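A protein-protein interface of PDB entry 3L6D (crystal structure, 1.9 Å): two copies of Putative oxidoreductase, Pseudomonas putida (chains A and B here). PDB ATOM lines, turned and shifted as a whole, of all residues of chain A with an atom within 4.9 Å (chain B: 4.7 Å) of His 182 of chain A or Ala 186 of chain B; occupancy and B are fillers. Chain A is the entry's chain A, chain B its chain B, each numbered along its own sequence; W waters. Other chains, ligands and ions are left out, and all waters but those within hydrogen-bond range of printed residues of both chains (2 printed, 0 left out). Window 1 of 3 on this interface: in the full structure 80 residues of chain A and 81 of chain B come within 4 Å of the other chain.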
ATOM      1  N   VAL A 178       6.874 -22.450  16.035  1.00  0.00           N
ATOM      2  CA  VAL A 178       7.424 -23.202  17.170  1.00  0.00           C
ATOM      3  C   VAL A 178       8.672 -24.001  16.793  1.00  0.00           C
ATOM      4  O   VAL A 178       9.606 -24.121  17.594  1.00  0.00           O
ATOM      5  CB  VAL A 178       6.343 -24.018  17.963  1.00  0.00           C
ATOM      6  CG1 VAL A 178       5.222 -23.093  18.423  1.00  0.00           C
ATOM      7  CG2 VAL A 178       5.786 -25.155  17.175  1.00  0.00           C
ATOM      8  N   LEU A 179       8.701 -24.540  15.580  1.00  0.00           N
ATOM      9  CA  LEU A 179       9.873 -25.251  15.123  1.00  0.00           C
ATOM     10  C   LEU A 179      11.091 -24.323  15.101  1.00  0.00           C
ATOM     11  O   LEU A 179      12.141 -24.727  15.561  1.00  0.00           O
ATOM     12  CB  LEU A 179       9.634 -25.878  13.741  1.00  0.00           C
ATOM     13  CG  LEU A 179      10.819 -26.489  12.999  1.00  0.00           C
ATOM     14  CD1 LEU A 179      10.992 -27.908  13.441  1.00  0.00           C
ATOM     15  CD2 LEU A 179      10.511 -26.430  11.490  1.00  0.00           C
ATOM     16  N   HIS A 180      10.964 -23.113  14.540  1.00  0.00           N
ATOM     17  CA  HIS A 180      12.101 -22.187  14.472  1.00  0.00           C
ATOM     18  C   HIS A 180      12.472 -21.582  15.825  1.00  0.00           C
ATOM     19  O   HIS A 180      13.672 -21.339  16.093  1.00  0.00           O
ATOM     20  CB  HIS A 180      11.895 -21.102  13.418  1.00  0.00           C
ATOM     21  CG  HIS A 180      11.967 -21.621  12.010  1.00  0.00           C
ATOM     22  ND1 HIS A 180      10.918 -22.287  11.405  1.00  0.00           N
ATOM     23  CD2 HIS A 180      12.958 -21.566  11.086  1.00  0.00           C
ATOM     24  CE1 HIS A 180      11.266 -22.626  10.171  1.00  0.00           C
ATOM     25  NE2 HIS A 180      12.503 -22.200   9.954  1.00  0.00           N
ATOM     26  N   ALA A 181      11.465 -21.356  16.677  1.00  0.00           N
ATOM     27  CA  ALA A 181      11.699 -20.942  18.040  1.00  0.00           C
ATOM     28  C   ALA A 181      12.679 -21.929  18.693  1.00  0.00           C
ATOM     29  O   ALA A 181      13.719 -21.502  19.159  1.00  0.00           O
ATOM     30  CB  ALA A 181      10.405 -20.885  18.824  1.00  0.00           C
ATOM     31  N   HIS A 182      12.360 -23.232  18.685  1.00  0.00           N
ATOM     32  CA  HIS A 182      13.262 -24.234  19.261  1.00  0.00           C
ATOM     33  C   HIS A 182      14.611 -24.235  18.547  1.00  0.00           C
ATOM     34  O   HIS A 182      15.657 -24.193  19.210  1.00  0.00           O
ATOM     35  CB  HIS A 182      12.664 -25.652  19.223  1.00  0.00           C
ATOM     36  CG  HIS A 182      13.685 -26.727  19.431  1.00  0.00           C
ATOM     37  ND1 HIS A 182      14.527 -26.741  20.522  1.00  0.00           N
ATOM     38  CD2 HIS A 182      14.020 -27.804  18.679  1.00  0.00           C
ATOM     39  CE1 HIS A 182      15.336 -27.787  20.439  1.00  0.00           C
ATOM     40  NE2 HIS A 182      15.046 -28.452  19.332  1.00  0.00           N
ATOM     41  N   ALA A 183      14.593 -24.371  17.218  1.00  0.00           N
ATOM     42  CA  ALA A 183      15.836 -24.501  16.447  1.00  0.00           C
ATOM     43  C   ALA A 183      16.810 -23.376  16.680  1.00  0.00           C
ATOM     44  O   ALA A 183      17.979 -23.602  16.992  1.00  0.00           O
ATOM     45  CB  ALA A 183      15.543 -24.634  14.947  1.00  0.00           C
ATOM     46  N   PHE A 184      16.325 -22.148  16.568  1.00  0.00           N
ATOM     47  CA  PHE A 184      17.172 -20.973  16.773  1.00  0.00           C
ATOM     48  C   PHE A 184      17.566 -20.782  18.247  1.00  0.00           C
ATOM     49  O   PHE A 184      18.706 -20.412  18.553  1.00  0.00           O
ATOM     50  CB  PHE A 184      16.464 -19.709  16.270  1.00  0.00           C
ATOM     51  CG  PHE A 184      16.358 -19.606  14.738  1.00  0.00           C
ATOM     52  CD1 PHE A 184      17.451 -19.919  13.903  1.00  0.00           C
ATOM     53  CD2 PHE A 184      15.176 -19.140  14.143  1.00  0.00           C
ATOM     54  CE1 PHE A 184      17.352 -19.787  12.490  1.00  0.00           C
ATOM     55  CE2 PHE A 184      15.064 -18.982  12.744  1.00  0.00           C
ATOM     56  CZ  PHE A 184      16.146 -19.320  11.905  1.00  0.00           C
ATOM     57  N   ALA A 185      16.639 -21.061  19.163  1.00  0.00           N
ATOM     58  CA  ALA A 185      16.997 -20.967  20.585  1.00  0.00           C
ATOM     59  C   ALA A 185      18.107 -21.978  20.938  1.00  0.00           C
ATOM     60  O   ALA A 185      19.046 -21.633  21.627  1.00  0.00           O
ATOM     61  CB  ALA A 185      15.756 -21.107  21.499  1.00  0.00           C
ATOM     62  N   ALA A 186      18.014 -23.205  20.426  1.00  0.00           N
ATOM     63  CA  ALA A 186      19.046 -24.228  20.707  1.00  0.00           C
ATOM     64  C   ALA A 186      20.443 -23.773  20.226  1.00  0.00           C
ATOM     65  O   ALA A 186      21.449 -23.930  20.947  1.00  0.00           O
ATOM     66  CB  ALA A 186      18.673 -25.535  20.052  1.00  0.00           C
ATOM     67  N   THR A 189      21.682 -21.093  22.783  1.00  0.00           N
ATOM     68  CA  THR A 189      22.156 -21.756  23.995  1.00  0.00           C
ATOM     69  C   THR A 189      23.600 -22.215  23.812  1.00  0.00           C
ATOM     70  O   THR A 189      24.422 -22.043  24.710  1.00  0.00           O
ATOM     71  CB  THR A 189      21.296 -22.967  24.486  1.00  0.00           C
ATOM     72  OG1 THR A 189      21.524 -24.120  23.670  1.00  0.00           O
ATOM     73  CG2 THR A 189      19.821 -22.619  24.528  1.00  0.00           C
ATOM     74  N   VAL A 219      22.084 -34.977  24.575  1.00  0.00           N
ATOM     75  CA  VAL A 219      20.930 -34.112  24.209  1.00  0.00           C
ATOM     76  C   VAL A 219      19.962 -34.898  23.283  1.00  0.00           C
ATOM     77  O   VAL A 219      18.762 -34.998  23.570  1.00  0.00           O
ATOM     78  CB  VAL A 219      21.407 -32.786  23.501  1.00  0.00           C
ATOM     79  CG1 VAL A 219      20.243 -32.030  22.829  1.00  0.00           C
ATOM     80  CG2 VAL A 219      22.163 -31.851  24.481  1.00  0.00           C
ATOM     81  N   LEU A 223      16.112 -35.727  24.225  1.00  0.00           N
ATOM     82  CA  LEU A 223      14.958 -35.295  23.413  1.00  0.00           C
ATOM     83  C   LEU A 223      14.103 -36.456  22.869  1.00  0.00           C
ATOM     84  O   LEU A 223      12.878 -36.338  22.843  1.00  0.00           O
ATOM     85  CB  LEU A 223      15.379 -34.356  22.274  1.00  0.00           C
ATOM     86  CG  LEU A 223      16.126 -33.042  22.604  1.00  0.00           C
ATOM     87  CD1 LEU A 223      16.520 -32.316  21.305  1.00  0.00           C
ATOM     88  CD2 LEU A 223      15.302 -32.148  23.518  1.00  0.00           C
ATOM     89  N   HIS B 182      24.566 -25.756  28.359  1.00  0.00           N
ATOM     90  CA  HIS B 182      24.080 -25.924  26.990  1.00  0.00           C
ATOM     91  C   HIS B 182      23.119 -27.093  26.844  1.00  0.00           C
ATOM     92  O   HIS B 182      22.033 -26.935  26.226  1.00  0.00           O
ATOM     93  CB  HIS B 182      25.215 -26.055  25.979  1.00  0.00           C
ATOM     94  CG  HIS B 182      24.774 -26.607  24.656  1.00  0.00           C
ATOM     95  ND1 HIS B 182      23.766 -26.027  23.906  1.00  0.00           N
ATOM     96  CD2 HIS B 182      25.168 -27.708  23.974  1.00  0.00           C
ATOM     97  CE1 HIS B 182      23.576 -26.743  22.809  1.00  0.00           C
ATOM     98  NE2 HIS B 182      24.424 -27.755  22.818  1.00  0.00           N
ATOM     99  N   ALA B 183      23.485 -28.233  27.426  1.00  0.00           N
ATOM    100  CA  ALA B 183      22.732 -29.478  27.199  1.00  0.00           C
ATOM    101  C   ALA B 183      21.362 -29.331  27.804  1.00  0.00           C
ATOM    102  O   ALA B 183      20.349 -29.634  27.150  1.00  0.00           O
ATOM    103  CB  ALA B 183      23.469 -30.699  27.789  1.00  0.00           C
ATOM    104  N   PHE B 184      21.314 -28.814  29.028  1.00  0.00           N
ATOM    105  CA  PHE B 184      20.019 -28.665  29.707  1.00  0.00           C
ATOM    106  C   PHE B 184      19.198 -27.536  29.104  1.00  0.00           C
ATOM    107  O   PHE B 184      17.990 -27.669  28.958  1.00  0.00           O
ATOM    108  CB  PHE B 184      20.175 -28.437  31.196  1.00  0.00           C
ATOM    109  CG  PHE B 184      20.683 -29.625  31.939  1.00  0.00           C
ATOM    110  CD1 PHE B 184      20.116 -30.886  31.752  1.00  0.00           C
ATOM    111  CD2 PHE B 184      21.725 -29.494  32.860  1.00  0.00           C
ATOM    112  CE1 PHE B 184      20.580 -31.995  32.461  1.00  0.00           C
ATOM    113  CE2 PHE B 184      22.185 -30.598  33.609  1.00  0.00           C
ATOM    114  CZ  PHE B 184      21.624 -31.848  33.401  1.00  0.00           C
ATOM    115  N   ALA B 185      19.847 -26.436  28.734  1.00  0.00           N
ATOM    116  CA  ALA B 185      19.110 -25.356  28.087  1.00  0.00           C
ATOM    117  C   ALA B 185      18.473 -25.800  26.763  1.00  0.00           C
ATOM    118  O   ALA B 185      17.341 -25.442  26.466  1.00  0.00           O
ATOM    119  CB  ALA B 185      19.994 -24.134  27.874  1.00  0.00           C
ATOM    120  N   ALA B 186      19.215 -26.579  25.987  1.00  0.00           N
ATOM    121  CA  ALA B 186      18.728 -27.099  24.698  1.00  0.00           C
ATOM    122  C   ALA B 186      17.471 -27.926  24.920  1.00  0.00           C
ATOM    123  O   ALA B 186      16.486 -27.753  24.203  1.00  0.00           O
ATOM    124  CB  ALA B 186      19.805 -27.921  24.022  1.00  0.00           C
ATOM    125  N   MET B 187      17.482 -28.793  25.923  1.00  0.00           N
ATOM    126  CA  MET B 187      16.276 -29.550  26.282  1.00  0.00           C
ATOM    127  C   MET B 187      15.095 -28.662  26.622  1.00  0.00           C
ATOM    128  O   MET B 187      13.966 -28.915  26.153  1.00  0.00           O
ATOM    129  CB  MET B 187      16.556 -30.485  27.463  1.00  0.00           C
ATOM    130  CG  MET B 187      17.623 -31.535  27.148  1.00  0.00           C
ATOM    131  SD  MET B 187      18.086 -32.543  28.768  1.00  0.00           S
ATOM    132  CE  MET B 187      16.331 -32.941  29.496  1.00  0.00           C
ATOM    133  N   VAL B 188      15.337 -27.652  27.461  1.00  0.00           N
ATOM    134  CA  VAL B 188      14.262 -26.774  27.888  1.00  0.00           C
ATOM    135  C   VAL B 188      13.677 -25.932  26.708  1.00  0.00           C
ATOM    136  O   VAL B 188      12.463 -25.725  26.657  1.00  0.00           O
ATOM    137  CB  VAL B 188      14.680 -25.947  29.115  1.00  0.00           C
ATOM    138  CG1 VAL B 188      13.643 -24.877  29.439  1.00  0.00           C
ATOM    139  CG2 VAL B 188      14.921 -26.894  30.327  1.00  0.00           C
ATOM    140  N   THR B 189      14.517 -25.510  25.751  1.00  0.00           N
ATOM    141  CA  THR B 189      14.007 -24.792  24.573  1.00  0.00           C
ATOM    142  C   THR B 189      13.029 -25.674  23.832  1.00  0.00           C
ATOM    143  O   THR B 189      12.027 -25.187  23.289  1.00  0.00           O
ATOM    144  CB  THR B 189      15.105 -24.318  23.551  1.00  0.00           C
ATOM    145  OG1 THR B 189      15.734 -25.453  22.925  1.00  0.00           O
ATOM    146  CG2 THR B 189      16.151 -23.406  24.214  1.00  0.00           C
ATOM    147  N   PHE B 190      13.302 -26.976  23.841  1.00  0.00           N
ATOM    148  CA  PHE B 190      12.398 -27.906  23.206  1.00  0.00           C
ATOM    149  C   PHE B 190      11.063 -27.994  23.961  1.00  0.00           C
ATOM    150  O   PHE B 190      10.003 -27.907  23.337  1.00  0.00           O
ATOM    151  CB  PHE B 190      13.073 -29.278  23.004  1.00  0.00           C
ATOM    152  CG  PHE B 190      12.209 -30.279  22.311  1.00  0.00           C
ATOM    153  CD1 PHE B 190      12.168 -30.337  20.919  1.00  0.00           C
ATOM    154  CD2 PHE B 190      11.425 -31.184  23.056  1.00  0.00           C
ATOM    155  CE1 PHE B 190      11.349 -31.262  20.271  1.00  0.00           C
ATOM    156  CE2 PHE B 190      10.600 -32.128  22.412  1.00  0.00           C
ATOM    157  CZ  PHE B 190      10.557 -32.162  21.015  1.00  0.00           C
ATOM    158  N   ALA B 193       8.985 -24.829  23.277  1.00  0.00           N
ATOM    159  CA  ALA B 193       8.420 -24.729  21.924  1.00  0.00           C
ATOM    160  C   ALA B 193       7.256 -25.680  21.773  1.00  0.00           C
ATOM    161  O   ALA B 193       6.203 -25.296  21.250  1.00  0.00           O
ATOM    162  CB  ALA B 193       9.493 -24.982  20.851  1.00  0.00           C
ATOM    163  N   LEU B 211       8.262 -32.041  15.678  1.00  0.00           N
ATOM    164  CA  LEU B 211       9.157 -30.918  15.933  1.00  0.00           C
ATOM    165  C   LEU B 211      10.604 -31.408  15.998  1.00  0.00           C
ATOM    166  O   LEU B 211      11.485 -30.861  15.343  1.00  0.00           O
ATOM    167  CB  LEU B 211       8.775 -30.164  17.222  1.00  0.00           C
ATOM    168  CG  LEU B 211       9.073 -28.652  17.208  1.00  0.00           C
ATOM    169  CD1 LEU B 211       8.281 -27.879  18.270  1.00  0.00           C
ATOM    170  CD2 LEU B 211      10.551 -28.374  17.375  1.00  0.00           C
ATOM    171  N   SER B 215      13.491 -30.579  12.895  1.00  0.00           N
ATOM    172  CA  SER B 215      14.567 -29.662  13.282  1.00  0.00           C
ATOM    173  C   SER B 215      15.937 -30.320  13.459  1.00  0.00           C
ATOM    174  O   SER B 215      16.944 -29.626  13.422  1.00  0.00           O
ATOM    175  CB  SER B 215      14.214 -28.944  14.579  1.00  0.00           C
ATOM    176  OG  SER B 215      14.196 -29.869  15.661  1.00  0.00           O
HETATM  177  O   HOH W   1      11.999 -22.528  22.058  1.00  0.00           O
HETATM  178  O   HOH W   2      15.975 -30.466  17.595  1.00  0.00           O
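ND1 of His 182 of chain A lies within hydrogen-bond range of OG1 of Thr 189 of chain B (3.0 Å). OG1 of Thr 189 of chain A is in hydrogen-bond range of ND1 of His 182 of chain B.
The backbone carbonyl oxygen of Ala 186 of chain A lies within hydrogen-bond range of the side-chain hydroxyl of Thr 189 of chain A (2.7 Å). The backbone carbonyl oxygen (O) of Ala 186 of chain B lies within hydrogen-bond range of the side-chain hydroxyl (OG1) of Thr 189 of chain B. The backbone carbonyl oxygen of Leu 211 of chain B sits at hydrogen-bond distance from the side-chain hydroxyl of Ser 215 of chain B (2.9 Å).
Val 178 of chain A touches Leu 211 of chain B (CG2 to CD1, 3.9 Å). CD1 of Leu 179 of chain A touches O of Leu 211 of chain B (3.5 Å). Leu 179 of chain A touches Ser 215 of chain B (CD1 to CB, 3.6 Å). His 182 of chain A touches Ala 186 of chain B (CE1 to O, 3.9 Å). N of Phe 190 of chain B touches ND1 of His 182 of chain A, at 3.5 Å. His 182 of chain A touches Ala 193 of chain B. Leu 211 of chain B touches His 182 of chain A. Ser 215 of chain B touches His 182 of chain A. Ala 186 of chain A touches His 182 of chain B (O to CE1, 3.99 Å). CD2 of Leu 223 of chain A touches CA of Met 187 of chain B, at 3.9 Å.
His 182 of chain A touches just these residues of chain B: Ala 186, Thr 189, Phe 190, Ala 193, Leu 211 and Ser 215. Ala 186 of chain B touches one residue of chain A. Of the printed residues of chain A, Met 187 of chain B touches Leu 223 (3.9 Å). Printed residues of chain B within 4 Å of Ala 185 of chain A: Thr 189. Of the printed residues of chain A, Thr 189 of chain B touches His 182, Ala 185 and Thr 189. The nearest residue of chain A that does not touch Ala 186 of chain B is Thr 189 of chain A (4.1 Å). The nearest printed residue of chain B that does not touch Leu 179 of chain A is Ala 193 of chain B (5.3 Å).
Hydrophobic or aromatic side chains of chain A that line the printed part of chain B: Val 178, Leu 179, His 182, Ala 185, Val 219 and Leu 223. Along chain A the printed residues that touch a printed residue of chain B span positions 178 to 223. Printed residues of chain B that touch a printed residue of chain A: His 182, Ala 183, Ala 185, Ala 186, Met 187, Thr 189, Phe 190, Ala 193, Leu 211 and Ser 215. Hydrophobic or aromatic side chains of chain B within 4 Å of the printed part of chain A: His 182, Ala 183, Ala 185, Phe 190, Ala 193 and Leu 211.
His 182 of chain A touches Ala 186 of chain B, and with the chains exchanged Ala 186 of chain A touches His 182 of chain B. His 182 of chain A touches Thr 189 of chain B, and with the chains exchanged Thr 189 of chain A touches His 182 of chain B. Ala 185 of chain A touches Thr 189 of chain B, and with the chains exchanged Thr 189 of chain A touches Ala 185 of chain B. Thr 189 of chain A touches its own counterpart, Thr 189 of chain B. 6 positions are printed for both chains.
Water W2 lies within hydrogen-bond range of the side-chain hydroxyl of Ser 215 of chain B (2.7 Å) and a ring nitrogen (NE2) of His 182 of chain A (2.8 Å). Water W1 bridges O of Thr 189 of chain B (2.9 Å) and N of His 182 of chain A (3.5 Å).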
